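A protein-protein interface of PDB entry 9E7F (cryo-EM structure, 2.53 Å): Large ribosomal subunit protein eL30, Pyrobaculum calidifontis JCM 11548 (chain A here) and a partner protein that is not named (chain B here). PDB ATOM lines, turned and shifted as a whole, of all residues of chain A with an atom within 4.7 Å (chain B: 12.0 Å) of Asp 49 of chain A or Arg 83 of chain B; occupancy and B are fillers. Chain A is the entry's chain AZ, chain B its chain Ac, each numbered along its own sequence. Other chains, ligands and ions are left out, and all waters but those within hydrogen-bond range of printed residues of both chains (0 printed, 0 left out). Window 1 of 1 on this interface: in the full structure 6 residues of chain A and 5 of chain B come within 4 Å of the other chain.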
ATOM      1  N   LYS A  25      23.010  18.697  19.280  1.00  0.00           N
ATOM      2  CA  LYS A  25      22.664  19.218  17.964  1.00  0.00           C
ATOM      3  C   LYS A  25      23.780  20.091  17.415  1.00  0.00           C
ATOM      4  O   LYS A  25      24.079  20.051  16.217  1.00  0.00           O
ATOM      5  CB  LYS A  25      21.354  19.998  18.038  1.00  0.00           C
ATOM      6  CG  LYS A  25      20.125  19.167  17.731  1.00  0.00           C
ATOM      7  CD  LYS A  25      18.909  19.690  18.471  1.00  0.00           C
ATOM      8  CE  LYS A  25      19.116  21.122  18.928  1.00  0.00           C
ATOM      9  NZ  LYS A  25      18.081  21.552  19.908  1.00  0.00           N
ATOM     10  N   TRP A  45       9.683  15.797  18.454  1.00  0.00           N
ATOM     11  CA  TRP A  45      10.489  16.832  17.817  1.00  0.00           C
ATOM     12  C   TRP A  45      11.972  16.648  18.122  1.00  0.00           C
ATOM     13  O   TRP A  45      12.823  16.878  17.259  1.00  0.00           O
ATOM     14  CB  TRP A  45       9.999  18.224  18.242  1.00  0.00           C
ATOM     15  CG  TRP A  45      10.184  18.553  19.694  1.00  0.00           C
ATOM     16  CD1 TRP A  45       9.273  18.389  20.690  1.00  0.00           C
ATOM     17  CD2 TRP A  45      11.355  19.101  20.309  1.00  0.00           C
ATOM     18  NE1 TRP A  45       9.804  18.791  21.888  1.00  0.00           N
ATOM     19  CE2 TRP A  45      11.084  19.230  21.680  1.00  0.00           C
ATOM     20  CE3 TRP A  45      12.614  19.473  19.833  1.00  0.00           C
ATOM     21  CZ2 TRP A  45      12.019  19.731  22.579  1.00  0.00           C
ATOM     22  CZ3 TRP A  45      13.539  19.969  20.725  1.00  0.00           C
ATOM     23  CH2 TRP A  45      13.237  20.096  22.082  1.00  0.00           C
ATOM     24  N   ALA A  46      12.300  16.222  19.342  1.00  0.00           N
ATOM     25  CA  ALA A  46      13.700  16.063  19.709  1.00  0.00           C
ATOM     26  C   ALA A  46      14.282  14.810  19.081  1.00  0.00           C
ATOM     27  O   ALA A  46      15.454  14.786  18.693  1.00  0.00           O
ATOM     28  CB  ALA A  46      13.843  16.023  21.228  1.00  0.00           C
ATOM     29  N   ARG A  47      13.474  13.758  18.978  1.00  0.00           N
ATOM     30  CA  ARG A  47      13.937  12.538  18.337  1.00  0.00           C
ATOM     31  C   ARG A  47      14.183  12.763  16.853  1.00  0.00           C
ATOM     32  O   ARG A  47      15.274  12.479  16.353  1.00  0.00           O
ATOM     33  CB  ARG A  47      12.921  11.421  18.566  1.00  0.00           C
ATOM     34  CG  ARG A  47      13.264  10.104  17.915  1.00  0.00           C
ATOM     35  CD  ARG A  47      12.182   9.703  16.934  1.00  0.00           C
ATOM     36  NE  ARG A  47      10.849   9.948  17.467  1.00  0.00           N
ATOM     37  CZ  ARG A  47      10.003   8.998  17.840  1.00  0.00           C
ATOM     38  NH1 ARG A  47      10.321   7.717  17.755  1.00  0.00           N
ATOM     39  NH2 ARG A  47       8.805   9.340  18.305  1.00  0.00           N
ATOM     40  N   GLU A  48      13.206  13.333  16.145  1.00  0.00           N
ATOM     41  CA  GLU A  48      13.337  13.453  14.697  1.00  0.00           C
ATOM     42  C   GLU A  48      14.379  14.486  14.297  1.00  0.00           C
ATOM     43  O   GLU A  48      14.933  14.408  13.196  1.00  0.00           O
ATOM     44  CB  GLU A  48      11.988  13.786  14.061  1.00  0.00           C
ATOM     45  CG  GLU A  48      11.322  12.669  13.222  1.00  0.00           C
ATOM     46  CD  GLU A  48      12.224  11.931  12.206  1.00  0.00           C
ATOM     47  OE1 GLU A  48      11.687  11.046  11.507  1.00  0.00           O
ATOM     48  OE2 GLU A  48      13.428  12.226  12.048  1.00  0.00           O
ATOM     49  N   ASP A  49      14.657  15.464  15.160  1.00  0.00           N
ATOM     50  CA  ASP A  49      15.769  16.368  14.891  1.00  0.00           C
ATOM     51  C   ASP A  49      17.099  15.639  14.996  1.00  0.00           C
ATOM     52  O   ASP A  49      18.029  15.920  14.233  1.00  0.00           O
ATOM     53  CB  ASP A  49      15.739  17.558  15.849  1.00  0.00           C
ATOM     54  CG  ASP A  49      14.695  18.585  15.473  1.00  0.00           C
ATOM     55  OD1 ASP A  49      13.817  18.260  14.653  1.00  0.00           O
ATOM     56  OD2 ASP A  49      14.762  19.725  15.979  1.00  0.00           O
ATOM     57  N   ILE A  50      17.214  14.707  15.941  1.00  0.00           N
ATOM     58  CA  ILE A  50      18.476  14.001  16.137  1.00  0.00           C
ATOM     59  C   ILE A  50      18.760  13.072  14.965  1.00  0.00           C
ATOM     60  O   ILE A  50      19.881  13.038  14.445  1.00  0.00           O
ATOM     61  CB  ILE A  50      18.466  13.229  17.466  1.00  0.00           C
ATOM     62  CG1 ILE A  50      18.492  14.195  18.647  1.00  0.00           C
ATOM     63  CG2 ILE A  50      19.660  12.310  17.528  1.00  0.00           C
ATOM     64  CD1 ILE A  50      19.849  14.778  18.915  1.00  0.00           C
ATOM     65  N   GLU A  51      17.758  12.295  14.540  1.00  0.00           N
ATOM     66  CA  GLU A  51      17.973  11.342  13.455  1.00  0.00           C
ATOM     67  C   GLU A  51      18.277  12.044  12.143  1.00  0.00           C
ATOM     68  O   GLU A  51      19.106  11.569  11.360  1.00  0.00           O
ATOM     69  CB  GLU A  51      16.763  10.428  13.287  1.00  0.00           C
ATOM     70  CG  GLU A  51      15.951  10.225  14.531  1.00  0.00           C
ATOM     71  CD  GLU A  51      15.080   8.990  14.459  1.00  0.00           C
ATOM     72  OE1 GLU A  51      14.590   8.543  15.518  1.00  0.00           O
ATOM     73  OE2 GLU A  51      14.887   8.465  13.344  1.00  0.00           O
ATOM     74  N   TYR A  52      17.618  13.173  11.880  1.00  0.00           N
ATOM     75  CA  TYR A  52      17.814  13.848  10.604  1.00  0.00           C
ATOM     76  C   TYR A  52      19.212  14.445  10.514  1.00  0.00           C
ATOM     77  O   TYR A  52      19.890  14.305   9.491  1.00  0.00           O
ATOM     78  CB  TYR A  52      16.717  14.901  10.400  1.00  0.00           C
ATOM     79  CG  TYR A  52      16.887  15.825   9.205  1.00  0.00           C
ATOM     80  CD1 TYR A  52      17.566  17.035   9.305  1.00  0.00           C
ATOM     81  CD2 TYR A  52      16.400  15.458   7.965  1.00  0.00           C
ATOM     82  CE1 TYR A  52      17.722  17.852   8.219  1.00  0.00           C
ATOM     83  CE2 TYR A  52      16.560  16.265   6.871  1.00  0.00           C
ATOM     84  CZ  TYR A  52      17.218  17.462   7.000  1.00  0.00           C
ATOM     85  OH  TYR A  52      17.369  18.272   5.899  1.00  0.00           O
ATOM     86  N   TYR A  53      19.667  15.110  11.575  1.00  0.00           N
ATOM     87  CA  TYR A  53      21.022  15.649  11.567  1.00  0.00           C
ATOM     88  C   TYR A  53      22.048  14.527  11.610  1.00  0.00           C
ATOM     89  O   TYR A  53      23.114  14.627  10.995  1.00  0.00           O
ATOM     90  CB  TYR A  53      21.224  16.601  12.746  1.00  0.00           C
ATOM     91  CG  TYR A  53      20.336  17.821  12.722  1.00  0.00           C
ATOM     92  CD1 TYR A  53      19.813  18.300  11.535  1.00  0.00           C
ATOM     93  CD2 TYR A  53      20.013  18.490  13.894  1.00  0.00           C
ATOM     94  CE1 TYR A  53      18.996  19.401  11.509  1.00  0.00           C
ATOM     95  CE2 TYR A  53      19.194  19.599  13.877  1.00  0.00           C
ATOM     96  CZ  TYR A  53      18.690  20.050  12.678  1.00  0.00           C
ATOM     97  OH  TYR A  53      17.875  21.158  12.638  1.00  0.00           O
ATOM     98  N   HIS B  71       7.176  32.841  16.776  1.00  0.00           N
ATOM     99  CA  HIS B  71       8.379  32.422  16.070  1.00  0.00           C
ATOM    100  C   HIS B  71       8.697  30.958  16.335  1.00  0.00           C
ATOM    101  O   HIS B  71       9.305  30.295  15.489  1.00  0.00           O
ATOM    102  CB  HIS B  71       9.554  33.320  16.456  1.00  0.00           C
ATOM    103  CG  HIS B  71      10.111  33.045  17.816  1.00  0.00           C
ATOM    104  ND1 HIS B  71       9.483  33.448  18.974  1.00  0.00           N
ATOM    105  CD2 HIS B  71      11.243  32.414  18.203  1.00  0.00           C
ATOM    106  CE1 HIS B  71      10.201  33.071  20.015  1.00  0.00           C
ATOM    107  NE2 HIS B  71      11.275  32.443  19.574  1.00  0.00           N
ATOM    108  N   LYS B  72       8.280  30.433  17.487  1.00  0.00           N
ATOM    109  CA  LYS B  72       8.569  29.042  17.826  1.00  0.00           C
ATOM    110  C   LYS B  72       7.804  28.082  16.925  1.00  0.00           C
ATOM    111  O   LYS B  72       8.361  27.098  16.429  1.00  0.00           O
ATOM    112  CB  LYS B  72       8.226  28.784  19.290  1.00  0.00           C
ATOM    113  CG  LYS B  72       9.249  27.963  20.020  1.00  0.00           C
ATOM    114  CD  LYS B  72      10.300  28.850  20.641  1.00  0.00           C
ATOM    115  CE  LYS B  72       9.682  29.793  21.642  1.00  0.00           C
ATOM    116  NZ  LYS B  72       8.970  29.057  22.716  1.00  0.00           N
ATOM    117  N   VAL B  73       6.518  28.349  16.715  1.00  0.00           N
ATOM    118  CA  VAL B  73       5.710  27.496  15.855  1.00  0.00           C
ATOM    119  C   VAL B  73       6.153  27.620  14.407  1.00  0.00           C
ATOM    120  O   VAL B  73       6.160  26.635  13.662  1.00  0.00           O
ATOM    121  CB  VAL B  73       4.221  27.839  16.021  1.00  0.00           C
ATOM    122  CG1 VAL B  73       3.393  27.088  15.003  1.00  0.00           C
ATOM    123  CG2 VAL B  73       3.764  27.524  17.434  1.00  0.00           C
ATOM    124  N   LEU B  74       6.518  28.829  13.981  1.00  0.00           N
ATOM    125  CA  LEU B  74       6.885  29.039  12.585  1.00  0.00           C
ATOM    126  C   LEU B  74       8.193  28.343  12.245  1.00  0.00           C
ATOM    127  O   LEU B  74       8.298  27.670  11.215  1.00  0.00           O
ATOM    128  CB  LEU B  74       6.988  30.531  12.286  1.00  0.00           C
ATOM    129  CG  LEU B  74       7.452  30.866  10.869  1.00  0.00           C
ATOM    130  CD1 LEU B  74       6.370  30.548   9.859  1.00  0.00           C
ATOM    131  CD2 LEU B  74       7.864  32.311  10.770  1.00  0.00           C
ATOM    132  N   ALA B  75       9.205  28.508  13.095  1.00  0.00           N
ATOM    133  CA  ALA B  75      10.510  27.918  12.821  1.00  0.00           C
ATOM    134  C   ALA B  75      10.439  26.400  12.833  1.00  0.00           C
ATOM    135  O   ALA B  75      11.027  25.732  11.975  1.00  0.00           O
ATOM    136  CB  ALA B  75      11.531  28.415  13.840  1.00  0.00           C
ATOM    137  N   ARG B  76       9.713  25.838  13.799  1.00  0.00           N
ATOM    138  CA  ARG B  76       9.596  24.389  13.898  1.00  0.00           C
ATOM    139  C   ARG B  76       8.828  23.818  12.715  1.00  0.00           C
ATOM    140  O   ARG B  76       9.180  22.758  12.189  1.00  0.00           O
ATOM    141  CB  ARG B  76       8.927  24.013  15.219  1.00  0.00           C
ATOM    142  CG  ARG B  76       8.143  22.722  15.181  1.00  0.00           C
ATOM    143  CD  ARG B  76       9.050  21.516  15.162  1.00  0.00           C
ATOM    144  NE  ARG B  76      10.313  21.763  15.843  1.00  0.00           N
ATOM    145  CZ  ARG B  76      11.433  21.101  15.592  1.00  0.00           C
ATOM    146  NH1 ARG B  76      11.480  20.143  14.683  1.00  0.00           N
ATOM    147  NH2 ARG B  76      12.535  21.411  16.267  1.00  0.00           N
ATOM    148  N   ALA B  77       7.771  24.508  12.285  1.00  0.00           N
ATOM    149  CA  ALA B  77       6.997  24.033  11.145  1.00  0.00           C
ATOM    150  C   ALA B  77       7.830  24.045   9.875  1.00  0.00           C
ATOM    151  O   ALA B  77       7.724  23.132   9.049  1.00  0.00           O
ATOM    152  CB  ALA B  77       5.738  24.878  10.971  1.00  0.00           C
ATOM    153  N   ILE B  78       8.673  25.065   9.711  1.00  0.00           N
ATOM    154  CA  ILE B  78       9.553  25.143   8.549  1.00  0.00           C
ATOM    155  C   ILE B  78      10.554  24.000   8.557  1.00  0.00           C
ATOM    156  O   ILE B  78      10.935  23.486   7.500  1.00  0.00           O
ATOM    157  CB  ILE B  78      10.264  26.506   8.508  1.00  0.00           C
ATOM    158  CG1 ILE B  78       9.257  27.628   8.272  1.00  0.00           C
ATOM    159  CG2 ILE B  78      11.334  26.514   7.435  1.00  0.00           C
ATOM    160  CD1 ILE B  78       9.849  29.003   8.426  1.00  0.00           C
ATOM    161  N   ARG B  79      11.014  23.600   9.745  1.00  0.00           N
ATOM    162  CA  ARG B  79      11.921  22.463   9.846  1.00  0.00           C
ATOM    163  C   ARG B  79      11.254  21.180   9.370  1.00  0.00           C
ATOM    164  O   ARG B  79      11.875  20.368   8.679  1.00  0.00           O
ATOM    165  CB  ARG B  79      12.402  22.305  11.286  1.00  0.00           C
ATOM    166  CG  ARG B  79      13.512  23.253  11.683  1.00  0.00           C
ATOM    167  CD  ARG B  79      14.170  22.808  12.976  1.00  0.00           C
ATOM    168  NE  ARG B  79      14.623  23.935  13.779  1.00  0.00           N
ATOM    169  CZ  ARG B  79      15.762  24.584  13.584  1.00  0.00           C
ATOM    170  NH1 ARG B  79      16.595  24.242  12.618  1.00  0.00           N
ATOM    171  NH2 ARG B  79      16.072  25.602  14.380  1.00  0.00           N
ATOM    172  N   TYR B  80       9.989  20.979   9.741  1.00  0.00           N
ATOM    173  CA  TYR B  80       9.265  19.793   9.299  1.00  0.00           C
ATOM    174  C   TYR B  80       9.056  19.805   7.793  1.00  0.00           C
ATOM    175  O   TYR B  80       9.172  18.766   7.135  1.00  0.00           O
ATOM    176  CB  TYR B  80       7.918  19.702  10.013  1.00  0.00           C
ATOM    177  CG  TYR B  80       7.989  19.194  11.431  1.00  0.00           C
ATOM    178  CD1 TYR B  80       9.172  18.716  11.961  1.00  0.00           C
ATOM    179  CD2 TYR B  80       6.864  19.192  12.235  1.00  0.00           C
ATOM    180  CE1 TYR B  80       9.231  18.251  13.255  1.00  0.00           C
ATOM    181  CE2 TYR B  80       6.912  18.729  13.528  1.00  0.00           C
ATOM    182  CZ  TYR B  80       8.096  18.260  14.034  1.00  0.00           C
ATOM    183  OH  TYR B  80       8.137  17.798  15.328  1.00  0.00           O
ATOM    184  N   ALA B  81       8.732  20.968   7.233  1.00  0.00           N
ATOM    185  CA  ALA B  81       8.513  21.058   5.795  1.00  0.00           C
ATOM    186  C   ALA B  81       9.797  20.797   5.023  1.00  0.00           C
ATOM    187  O   ALA B  81       9.762  20.279   3.902  1.00  0.00           O
ATOM    188  CB  ALA B  81       7.940  22.429   5.441  1.00  0.00           C
ATOM    189  N   VAL B  82      10.942  21.154   5.605  1.00  0.00           N
ATOM    190  CA  VAL B  82      12.221  20.936   4.937  1.00  0.00           C
ATOM    191  C   VAL B  82      12.510  19.445   4.817  1.00  0.00           C
ATOM    192  O   VAL B  82      12.963  18.963   3.774  1.00  0.00           O
ATOM    193  CB  VAL B  82      13.345  21.671   5.683  1.00  0.00           C
ATOM    194  CG1 VAL B  82      14.687  21.070   5.336  1.00  0.00           C
ATOM    195  CG2 VAL B  82      13.315  23.144   5.352  1.00  0.00           C
ATOM    196  N   ARG B  83      12.269  18.696   5.889  1.00  0.00           N
ATOM    197  CA  ARG B  83      12.515  17.261   5.856  1.00  0.00           C
ATOM    198  C   ARG B  83      11.419  16.500   5.127  1.00  0.00           C
ATOM    199  O   ARG B  83      11.695  15.469   4.506  1.00  0.00           O
ATOM    200  CB  ARG B  83      12.662  16.724   7.275  1.00  0.00           C
ATOM    201  CG  ARG B  83      13.667  17.489   8.090  1.00  0.00           C
ATOM    202  CD  ARG B  83      13.591  17.119   9.541  1.00  0.00           C
ATOM    203  NE  ARG B  83      14.162  18.163  10.377  1.00  0.00           N
ATOM    204  CZ  ARG B  83      13.883  18.323  11.660  1.00  0.00           C
ATOM    205  NH1 ARG B  83      13.046  17.517  12.289  1.00  0.00           N
ATOM    206  NH2 ARG B  83      14.459  19.314  12.329  1.00  0.00           N
ATOM    207  N   ARG B  84      10.185  16.979   5.199  1.00  0.00           N
ATOM    208  CA  ARG B  84       9.047  16.287   4.610  1.00  0.00           C
ATOM    209  C   ARG B  84       9.050  16.422   3.096  1.00  0.00           C
ATOM    210  O   ARG B  84      10.003  16.014   2.435  1.00  0.00           O
ATOM    211  CB  ARG B  84       7.748  16.836   5.195  1.00  0.00           C
ATOM    212  CG  ARG B  84       6.595  15.858   5.214  1.00  0.00           C
ATOM    213  CD  ARG B  84       5.756  16.041   6.467  1.00  0.00           C
ATOM    214  NE  ARG B  84       6.307  15.311   7.604  1.00  0.00           N
ATOM    215  CZ  ARG B  84       7.195  15.799   8.463  1.00  0.00           C
ATOM    216  NH1 ARG B  84       7.665  17.026   8.347  1.00  0.00           N
ATOM    217  NH2 ARG B  84       7.620  15.033   9.463  1.00  0.00           N
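The side-chain carboxylate (OD2) of Asp 49 of chain A lies within salt-bridge range of the guanidinium group (NH2) of Arg 76 of chain B, at 2.8 Å. OH of Tyr 53 of chain A is in hydrogen-bond range of NH1 of Arg 79 of chain B (3.3 Å). NH1 of Arg 83 of chain B lies within salt-bridge range of OD1 of Asp 49 of chain A.
O of Tyr 80 of chain B lies within hydrogen-bond range of NH1 of Arg 84 of chain B (2.6 Å).
Tyr 80 of chain B touches Trp 45 of chain A. Arg 83 of chain B touches Glu 48 of chain A (NH1 to O, 3.7 Å). OH of Tyr 52 of chain A touches CG1 of Val 82 of chain B (3.9 Å). Arg 83 of chain B touches Tyr 52 of chain A (CG to CE2, 3.4 Å). Tyr 53 of chain A touches Arg 83 of chain B.
No residue of chain B comes within 4 Å of Lys 25 of chain A. Of chain B, only Tyr 80 comes within 4 Å of Trp 45 of chain A. No residue of chain B comes within 4 Å of Ala 46 of chain A. Asp 49 of chain A touches just these residues of chain B: Arg 76 and Arg 83. No residue of chain B comes within 4 Å of Glu 51 of chain A. Of the printed residues of chain B, Tyr 52 of chain A touches Val 82 (3.9 Å) and Arg 83 (3.4 Å). Of the printed residues of chain A, Arg 76 of chain B touches Asp 49 (2.8 Å). Ile 78 of chain B touches none of the printed residues of chain A. Printed residues of chain A within 4 Å of Arg 79 of chain B: Tyr 53 (3.3 Å). Printed residues of chain A within 4 Å of Tyr 80 of chain B: Trp 45 (3.5 Å). Arg 83 of chain B touches just these residues of chain A: Glu 48, Asp 49, Tyr 52 and Tyr 53.
Of the 10 printed residues of chain A, 5 touch a printed residue of chain B. Hydrophobic or aromatic side chains of chain A within 4 Å of the printed part of chain B: Trp 45, Tyr 52 and Tyr 53. Along chain A the printed residues that touch a printed residue of chain B span positions 45 to 53. Of the 14 printed residues of chain B, 5 touch a printed residue of chain A. Hydrophobic or aromatic side chains of chain B within 4 Å of the printed part of chain A: Tyr 80 and Val 82. Among the printed residues, 8 pairs touch across the chains. Among the printed residues, Asp or Glu carboxylates within 4 Å of a Lys or Arg side-chain nitrogen of the other chain: Asp 49 of chain A with Arg 76 of chain B and Asp 49 of chain A with Arg 83 of chain B.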
